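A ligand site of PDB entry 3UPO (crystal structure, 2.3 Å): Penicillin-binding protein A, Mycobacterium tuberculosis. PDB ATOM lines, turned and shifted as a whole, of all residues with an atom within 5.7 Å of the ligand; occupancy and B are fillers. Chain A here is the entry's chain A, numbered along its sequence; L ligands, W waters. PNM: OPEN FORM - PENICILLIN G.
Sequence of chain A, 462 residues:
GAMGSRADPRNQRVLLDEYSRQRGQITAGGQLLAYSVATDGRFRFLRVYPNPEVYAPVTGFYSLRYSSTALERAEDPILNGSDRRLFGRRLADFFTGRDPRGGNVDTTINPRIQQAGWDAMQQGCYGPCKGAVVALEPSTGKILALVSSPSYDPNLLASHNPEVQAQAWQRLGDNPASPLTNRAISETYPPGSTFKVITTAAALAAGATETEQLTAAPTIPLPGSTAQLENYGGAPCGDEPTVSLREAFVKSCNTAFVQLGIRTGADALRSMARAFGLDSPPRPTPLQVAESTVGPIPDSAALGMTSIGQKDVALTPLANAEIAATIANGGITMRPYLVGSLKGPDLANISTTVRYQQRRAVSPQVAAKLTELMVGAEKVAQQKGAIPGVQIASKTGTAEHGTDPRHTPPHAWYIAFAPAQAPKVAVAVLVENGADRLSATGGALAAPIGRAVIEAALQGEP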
ATOM      1  N   PRO A 191     -25.641 -21.550  16.844  1.00  0.00           N
ATOM      2  CA  PRO A 191     -24.585 -22.277  17.568  1.00  0.00           C
ATOM      3  C   PRO A 191     -24.521 -21.931  19.080  1.00  0.00           C
ATOM      4  O   PRO A 191     -23.913 -22.675  19.843  1.00  0.00           O
ATOM      5  CB  PRO A 191     -23.303 -21.781  16.893  1.00  0.00           C
ATOM      6  CG  PRO A 191     -23.622 -20.411  16.425  1.00  0.00           C
ATOM      7  CD  PRO A 191     -25.078 -20.482  15.992  1.00  0.00           C
ATOM      8  N   GLY A 192     -25.115 -20.804  19.471  1.00  0.00           N
ATOM      9  CA  GLY A 192     -24.984 -20.324  20.837  1.00  0.00           C
ATOM     10  C   GLY A 192     -23.524 -20.155  21.225  1.00  0.00           C
ATOM     11  O   GLY A 192     -22.716 -19.645  20.434  1.00  0.00           O
ATOM     12  N   SER A 193     -23.156 -20.609  22.419  1.00  0.00           N
ATOM     13  CA  SER A 193     -21.847 -20.291  22.973  1.00  0.00           C
ATOM     14  C   SER A 193     -20.687 -21.071  22.408  1.00  0.00           C
ATOM     15  O   SER A 193     -19.536 -20.792  22.747  1.00  0.00           O
ATOM     16  CB  SER A 193     -21.841 -20.388  24.501  1.00  0.00           C
ATOM     17  OG  SER A 193     -22.801 -19.506  25.049  1.00  0.00           O
ATOM     18  N   THR A 194     -20.953 -22.062  21.557  1.00  0.00           N
ATOM     19  CA  THR A 194     -19.857 -22.656  20.798  1.00  0.00           C
ATOM     20  C   THR A 194     -19.184 -21.560  19.948  1.00  0.00           C
ATOM     21  O   THR A 194     -18.012 -21.641  19.645  1.00  0.00           O
ATOM     22  CB  THR A 194     -20.323 -23.839  19.904  1.00  0.00           C
ATOM     23  OG1 THR A 194     -21.360 -23.391  19.017  1.00  0.00           O
ATOM     24  CG2 THR A 194     -20.835 -25.017  20.765  1.00  0.00           C
ATOM     25  N   LYS A 196     -18.404 -18.658  20.786  1.00  0.00           N
ATOM     26  CA  LYS A 196     -17.385 -17.952  21.566  1.00  0.00           C
ATOM     27  C   LYS A 196     -15.994 -18.322  21.062  1.00  0.00           C
ATOM     28  O   LYS A 196     -15.041 -17.579  21.274  1.00  0.00           O
ATOM     29  CB  LYS A 196     -17.560 -18.202  23.065  1.00  0.00           C
ATOM     30  CG  LYS A 196     -18.799 -17.514  23.627  1.00  0.00           C
ATOM     31  CD  LYS A 196     -19.054 -17.885  25.064  1.00  0.00           C
ATOM     32  CE  LYS A 196     -20.196 -17.067  25.643  1.00  0.00           C
ATOM     33  NZ  LYS A 196     -20.730 -17.609  26.925  1.00  0.00           N
ATOM     34  N   GLU A 230     -28.070 -11.231  29.876  1.00  0.00           N
ATOM     35  CA  GLU A 230     -27.566 -11.669  31.176  1.00  0.00           C
ATOM     36  C   GLU A 230     -26.726 -12.957  31.092  1.00  0.00           C
ATOM     37  O   GLU A 230     -26.809 -13.694  30.117  1.00  0.00           O
ATOM     38  CB  GLU A 230     -28.715 -11.778  32.196  1.00  0.00           C
ATOM     39  CG  GLU A 230     -29.436 -13.110  32.252  1.00  0.00           C
ATOM     40  CD  GLU A 230     -30.379 -13.245  33.461  1.00  0.00           C
ATOM     41  OE1 GLU A 230     -30.739 -14.403  33.798  1.00  0.00           O
ATOM     42  OE2 GLU A 230     -30.779 -12.212  34.057  1.00  0.00           O
ATOM     43  N   ASN A 231     -25.909 -13.194  32.111  1.00  0.00           N
ATOM     44  CA  ASN A 231     -25.234 -14.492  32.322  1.00  0.00           C
ATOM     45  C   ASN A 231     -26.234 -15.582  32.687  1.00  0.00           C
ATOM     46  O   ASN A 231     -27.305 -15.293  33.205  1.00  0.00           O
ATOM     47  CB  ASN A 231     -24.239 -14.376  33.481  1.00  0.00           C
ATOM     48  CG  ASN A 231     -22.954 -13.662  33.095  1.00  0.00           C
ATOM     49  OD1 ASN A 231     -22.623 -13.487  31.930  1.00  0.00           O
ATOM     50  ND2 ASN A 231     -22.201 -13.248  34.114  1.00  0.00           N
ATOM     51  N   TYR A 232     -25.883 -16.833  32.433  1.00  0.00           N
ATOM     52  CA  TYR A 232     -26.735 -17.978  32.799  1.00  0.00           C
ATOM     53  C   TYR A 232     -27.021 -17.988  34.302  1.00  0.00           C
ATOM     54  O   TYR A 232     -26.091 -18.014  35.131  1.00  0.00           O
ATOM     55  CB  TYR A 232     -26.107 -19.316  32.381  1.00  0.00           C
ATOM     56  CG  TYR A 232     -27.106 -20.462  32.294  1.00  0.00           C
ATOM     57  CD1 TYR A 232     -28.063 -20.505  31.270  1.00  0.00           C
ATOM     58  CD2 TYR A 232     -27.098 -21.490  33.231  1.00  0.00           C
ATOM     59  CE1 TYR A 232     -28.997 -21.556  31.181  1.00  0.00           C
ATOM     60  CE2 TYR A 232     -28.022 -22.546  33.155  1.00  0.00           C
ATOM     61  CZ  TYR A 232     -28.966 -22.568  32.129  1.00  0.00           C
ATOM     62  OH  TYR A 232     -29.885 -23.609  32.047  1.00  0.00           O
ATOM     63  N   LYS A 251     -15.651 -20.630  31.869  1.00  0.00           N
ATOM     64  CA  LYS A 251     -16.929 -20.607  32.576  1.00  0.00           C
ATOM     65  C   LYS A 251     -18.123 -20.310  31.637  1.00  0.00           C
ATOM     66  O   LYS A 251     -19.275 -20.540  32.008  1.00  0.00           O
ATOM     67  CB  LYS A 251     -16.889 -19.630  33.742  1.00  0.00           C
ATOM     68  CG  LYS A 251     -15.872 -20.030  34.814  1.00  0.00           C
ATOM     69  CD  LYS A 251     -16.174 -19.437  36.184  1.00  0.00           C
ATOM     70  CE  LYS A 251     -15.476 -18.125  36.419  1.00  0.00           C
ATOM     71  NZ  LYS A 251     -15.160 -17.962  37.881  1.00  0.00           N
ATOM     72  N   SER A 252     -17.812 -19.822  30.425  1.00  0.00           N
ATOM     73  CA  SER A 252     -18.807 -19.427  29.425  1.00  0.00           C
ATOM     74  C   SER A 252     -19.751 -18.351  29.950  1.00  0.00           C
ATOM     75  O   SER A 252     -20.993 -18.526  29.910  1.00  0.00           O
ATOM     76  CB  SER A 252     -19.605 -20.646  28.879  1.00  0.00           C
ATOM     77  OG  SER A 252     -20.174 -20.339  27.607  1.00  0.00           O
ATOM     78  N   ASN A 254     -21.550 -14.825  29.677  1.00  0.00           N
ATOM     79  CA  ASN A 254     -22.091 -14.148  28.504  1.00  0.00           C
ATOM     80  C   ASN A 254     -21.700 -12.689  28.332  1.00  0.00           C
ATOM     81  O   ASN A 254     -21.196 -12.299  27.280  1.00  0.00           O
ATOM     82  CB  ASN A 254     -23.624 -14.257  28.469  1.00  0.00           C
ATOM     83  CG  ASN A 254     -24.093 -15.659  28.149  1.00  0.00           C
ATOM     84  OD1 ASN A 254     -23.305 -16.517  27.748  1.00  0.00           O
ATOM     85  ND2 ASN A 254     -25.384 -15.889  28.341  1.00  0.00           N
ATOM     86  N   ILE A 308     -22.302 -14.150  21.109  1.00  0.00           N
ATOM     87  CA  ILE A 308     -22.583 -15.370  21.863  1.00  0.00           C
ATOM     88  C   ILE A 308     -23.365 -16.378  21.027  1.00  0.00           C
ATOM     89  O   ILE A 308     -24.024 -17.254  21.577  1.00  0.00           O
ATOM     90  CB  ILE A 308     -23.254 -15.072  23.229  1.00  0.00           C
ATOM     91  CG1 ILE A 308     -24.642 -14.442  23.047  1.00  0.00           C
ATOM     92  CG2 ILE A 308     -22.309 -14.216  24.096  1.00  0.00           C
ATOM     93  CD1 ILE A 308     -25.368 -14.114  24.345  1.00  0.00           C
ATOM     94  N   GLN A 310     -25.910 -16.014  18.833  1.00  0.00           N
ATOM     95  CA  GLN A 310     -27.343 -15.840  18.691  1.00  0.00           C
ATOM     96  C   GLN A 310     -27.640 -14.895  17.516  1.00  0.00           C
ATOM     97  O   GLN A 310     -26.934 -14.923  16.515  1.00  0.00           O
ATOM     98  CB  GLN A 310     -27.961 -15.375  20.000  1.00  0.00           C
ATOM     99  CG  GLN A 310     -27.700 -16.308  21.175  1.00  0.00           C
ATOM    100  CD  GLN A 310     -28.577 -17.568  21.197  1.00  0.00           C
ATOM    101  OE1 GLN A 310     -28.374 -18.430  22.062  1.00  0.00           O
ATOM    102  NE2 GLN A 310     -29.527 -17.686  20.270  1.00  0.00           N
ATOM    103  N   LYS A 395     -15.909 -27.053  23.676  1.00  0.00           N
ATOM    104  CA  LYS A 395     -16.723 -25.909  24.055  1.00  0.00           C
ATOM    105  C   LYS A 395     -18.188 -26.327  23.987  1.00  0.00           C
ATOM    106  O   LYS A 395     -18.644 -26.841  22.950  1.00  0.00           O
ATOM    107  CB  LYS A 395     -16.453 -24.694  23.168  1.00  0.00           C
ATOM    108  CG  LYS A 395     -17.228 -23.434  23.593  1.00  0.00           C
ATOM    109  CD  LYS A 395     -16.831 -22.983  25.029  1.00  0.00           C
ATOM    110  CE  LYS A 395     -17.670 -21.846  25.550  1.00  0.00           C
ATOM    111  NZ  LYS A 395     -18.933 -22.320  26.181  1.00  0.00           N
ATOM    112  N   THR A 396     -18.905 -26.140  25.100  1.00  0.00           N
ATOM    113  CA  THR A 396     -20.356 -26.393  25.165  1.00  0.00           C
ATOM    114  C   THR A 396     -21.139 -25.191  24.671  1.00  0.00           C
ATOM    115  O   THR A 396     -20.609 -24.083  24.548  1.00  0.00           O
ATOM    116  CB  THR A 396     -20.842 -26.706  26.605  1.00  0.00           C
ATOM    117  OG1 THR A 396     -20.493 -25.619  27.470  1.00  0.00           O
ATOM    118  CG2 THR A 396     -20.242 -28.011  27.111  1.00  0.00           C
ATOM    119  N   GLY A 397     -22.422 -25.410  24.403  1.00  0.00           N
ATOM    120  CA  GLY A 397     -23.318 -24.326  24.040  1.00  0.00           C
ATOM    121  C   GLY A 397     -24.755 -24.716  24.279  1.00  0.00           C
ATOM    122  O   GLY A 397     -25.109 -25.887  24.194  1.00  0.00           O
ATOM    123  N   THR A 398     -25.570 -23.736  24.606  1.00  0.00           N
ATOM    124  CA  THR A 398     -27.004 -23.903  24.671  1.00  0.00           C
ATOM    125  C   THR A 398     -27.649 -22.674  24.048  1.00  0.00           C
ATOM    126  O   THR A 398     -27.494 -21.554  24.527  1.00  0.00           O
ATOM    127  CB  THR A 398     -27.556 -24.373  26.101  1.00  0.00           C
ATOM    128  OG1 THR A 398     -28.594 -23.501  26.576  1.00  0.00           O
ATOM    129  CG2 THR A 398     -26.477 -24.451  27.136  1.00  0.00           C
ATOM    130  N   ALA A 399     -28.333 -22.913  22.926  1.00  0.00           N
ATOM    131  CA  ALA A 399     -28.773 -21.851  22.055  1.00  0.00           C
ATOM    132  C   ALA A 399     -30.279 -21.704  22.098  1.00  0.00           C
ATOM    133  O   ALA A 399     -31.007 -22.667  21.894  1.00  0.00           O
ATOM    134  CB  ALA A 399     -28.310 -22.139  20.637  1.00  0.00           C
ATOM    135  N   GLU A 400     -30.743 -20.481  22.381  1.00  0.00           N
ATOM    136  CA  GLU A 400     -32.150 -20.151  22.277  1.00  0.00           C
ATOM    137  C   GLU A 400     -32.539 -20.012  20.813  1.00  0.00           C
ATOM    138  O   GLU A 400     -31.703 -19.695  19.954  1.00  0.00           O
ATOM    139  CB  GLU A 400     -32.453 -18.856  23.043  1.00  0.00           C
ATOM    140  CG  GLU A 400     -32.409 -19.012  24.584  1.00  0.00           C
ATOM    141  CD  GLU A 400     -33.359 -18.048  25.313  1.00  0.00           C
ATOM    142  OE1 GLU A 400     -33.431 -16.869  24.899  1.00  0.00           O
ATOM    143  OE2 GLU A 400     -34.004 -18.479  26.306  1.00  0.00           O
ATOM    144  N   TRP A 413     -25.475 -27.968  22.546  1.00  0.00           N
ATOM    145  CA  TRP A 413     -24.375 -28.144  21.616  1.00  0.00           C
ATOM    146  C   TRP A 413     -23.117 -28.558  22.331  1.00  0.00           C
ATOM    147  O   TRP A 413     -22.873 -28.126  23.459  1.00  0.00           O
ATOM    148  CB  TRP A 413     -24.050 -26.826  20.951  1.00  0.00           C
ATOM    149  CG  TRP A 413     -24.814 -26.394  19.728  1.00  0.00           C
ATOM    150  CD1 TRP A 413     -25.775 -25.432  19.676  1.00  0.00           C
ATOM    151  CD2 TRP A 413     -24.591 -26.808  18.384  1.00  0.00           C
ATOM    152  NE1 TRP A 413     -26.189 -25.249  18.383  1.00  0.00           N
ATOM    153  CE2 TRP A 413     -25.470 -26.074  17.564  1.00  0.00           C
ATOM    154  CE3 TRP A 413     -23.733 -27.753  17.787  1.00  0.00           C
ATOM    155  CZ2 TRP A 413     -25.518 -26.229  16.169  1.00  0.00           C
ATOM    156  CZ3 TRP A 413     -23.781 -27.908  16.392  1.00  0.00           C
ATOM    157  CH2 TRP A 413     -24.674 -27.158  15.602  1.00  0.00           C
ATOM    158  N   THR A 441     -28.877 -28.093  28.792  1.00  0.00           N
ATOM    159  CA  THR A 441     -27.569 -27.490  28.524  1.00  0.00           C
ATOM    160  C   THR A 441     -26.690 -28.436  27.697  1.00  0.00           C
ATOM    161  O   THR A 441     -26.865 -29.667  27.742  1.00  0.00           O
ATOM    162  CB  THR A 441     -26.795 -27.090  29.817  1.00  0.00           C
ATOM    163  OG1 THR A 441     -26.528 -28.255  30.596  1.00  0.00           O
ATOM    164  CG2 THR A 441     -27.556 -26.060  30.659  1.00  0.00           C
ATOM    165  N   GLY A 442     -25.739 -27.857  26.972  1.00  0.00           N
ATOM    166  CA  GLY A 442     -24.773 -28.629  26.197  1.00  0.00           C
ATOM    167  C   GLY A 442     -23.951 -29.560  27.047  1.00  0.00           C
ATOM    168  O   GLY A 442     -23.733 -30.717  26.676  1.00  0.00           O
ATOM    169  N   GLY A 443     -23.485 -29.044  28.196  1.00  0.00           N
ATOM    170  CA  GLY A 443     -22.690 -29.827  29.150  1.00  0.00           C
ATOM    171  C   GLY A 443     -23.437 -31.047  29.658  1.00  0.00           C
ATOM    172  O   GLY A 443     -22.862 -32.128  29.776  1.00  0.00           O
HETATM  173  O8  PNM L   1     -24.485 -21.038  24.891  1.00  0.00           O
HETATM  174  C7  PNM L   1     -24.011 -20.043  25.451  1.00  0.00           C
HETATM  175  N4  PNM L   1     -23.126 -21.069  27.472  1.00  0.00           N
HETATM  176  C3  PNM L   1     -23.806 -22.272  27.900  1.00  0.00           C
HETATM  177  C11 PNM L   1     -22.930 -23.471  27.695  1.00  0.00           C
HETATM  178  O13 PNM L   1     -23.487 -24.563  27.443  1.00  0.00           O
HETATM  179  O12 PNM L   1     -21.691 -23.321  27.750  1.00  0.00           O
HETATM  180  C2  PNM L   1     -24.254 -22.008  29.352  1.00  0.00           C
HETATM  181  C10 PNM L   1     -25.503 -22.808  29.713  1.00  0.00           C
HETATM  182  C9  PNM L   1     -23.172 -22.304  30.380  1.00  0.00           C
HETATM  183  S1  PNM L   1     -24.663 -20.289  29.358  1.00  0.00           S
HETATM  184  C5  PNM L   1     -23.808 -19.856  27.858  1.00  0.00           C
HETATM  185  C6  PNM L   1     -24.679 -19.424  26.661  1.00  0.00           C
HETATM  186  N14 PNM L   1     -26.050 -19.892  26.694  1.00  0.00           N
HETATM  187  C15 PNM L   1     -27.118 -19.335  27.510  1.00  0.00           C
HETATM  188  O16 PNM L   1     -26.873 -17.963  27.733  1.00  0.00           O
HETATM  189  C17 PNM L   1     -28.495 -19.597  26.877  1.00  0.00           C
HETATM  190  C18 PNM L   1     -29.158 -18.305  26.464  1.00  0.00           C
HETATM  191  C19 PNM L   1     -30.097 -17.717  27.322  1.00  0.00           C
HETATM  192  C20 PNM L   1     -30.692 -16.497  26.932  1.00  0.00           C
HETATM  193  C21 PNM L   1     -30.347 -15.876  25.724  1.00  0.00           C
HETATM  194  C22 PNM L   1     -29.411 -16.466  24.876  1.00  0.00           C
HETATM  195  C23 PNM L   1     -28.818 -17.688  25.244  1.00  0.00           C
HETATM  196  O   HOH W   1     -23.177 -26.429  29.306  1.00  0.00           O
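O8 of the ligand sits close to N of Ser 193. The side-chain hydroxyl of Ser 193 is bonded to a carbon (C7) of the ligand (1.4 Å). OG1 of Thr 396 sits at hydrogen-bond distance from O12 of the ligand (2.6 Å). The side-chain amide nitrogen (ND2) of Asn 254 is in hydrogen-bond range of an oxygen (O16) of the ligand (2.6 Å). N of Thr 398 lies within hydrogen-bond range of O8 of the ligand, at 2.9 Å. O of Thr 398 lies within hydrogen-bond range of N14 of the ligand (3.1 Å). The side-chain hydroxyl (OG) of Ser 252 sits at hydrogen-bond distance from a nitrogen (N4) of the ligand, 3.0 Å away. The side-chain amino group (NZ) of Lys 395 lies within salt-bridge range of an oxygen (O12) of the ligand, at 3.3 Å. The backbone NH of Gly 397 is in hydrogen-bond range of an oxygen (O13) of the ligand (3.3 Å).
The side-chain amino group of Lys 196 is in hydrogen-bond range of the side-chain hydroxyl of Ser 193, at 3.4 Å. OD1 of Asn 254 is in hydrogen-bond range of NZ of Lys 196 (2.9 Å). O of Glu 230 sits at hydrogen-bond distance from ND2 of Asn 254 (3.2 Å). N of Asn 254 is in hydrogen-bond range of OD1 of Asn 231 (2.8 Å). The side-chain hydroxyl (OG) of Ser 252 sits at hydrogen-bond distance from the side-chain amino group (NZ) of Lys 395 (2.7 Å). OG of Ser 252 is in hydrogen-bond range of NZ of Lys 196 (2.9 Å). O of Gly 397 lies close to N of Gly 442, 3.5 Å away. O of Gly 397 sits at hydrogen-bond distance from N of Trp 413, at 2.7 Å.
Gly 192 touches the ligand (C to O8, 3.9 Å). NZ of Lys 196 touches C5 of the ligand (3.9 Å). CB of Tyr 232 touches S1 of the ligand, 3.5 Å away. OE1 of Gln 310 touches C23 of the ligand, 3.3 Å away. Glu 400 touches the ligand (OE1 to C21, 3.3 Å). Thr 441 touches the ligand (CG2 to C10, 3.96 Å). Within 4 Å of the ligand: Gly 192, Ser 193, Lys 196, Tyr 232, Ser 252, Asn 254, Gln 310, Lys 395, Thr 396, Gly 397, Thr 398, Glu 400 and Thr 441. The nearest printed residue that does not touch the ligand is Gly 442 (4.02 Å).
Water W1 lies within hydrogen-bond range of O13 of the ligand (2.7 Å), N of Gly 443 (2.9 Å) and OG1 of Thr 396 (3.4 Å).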
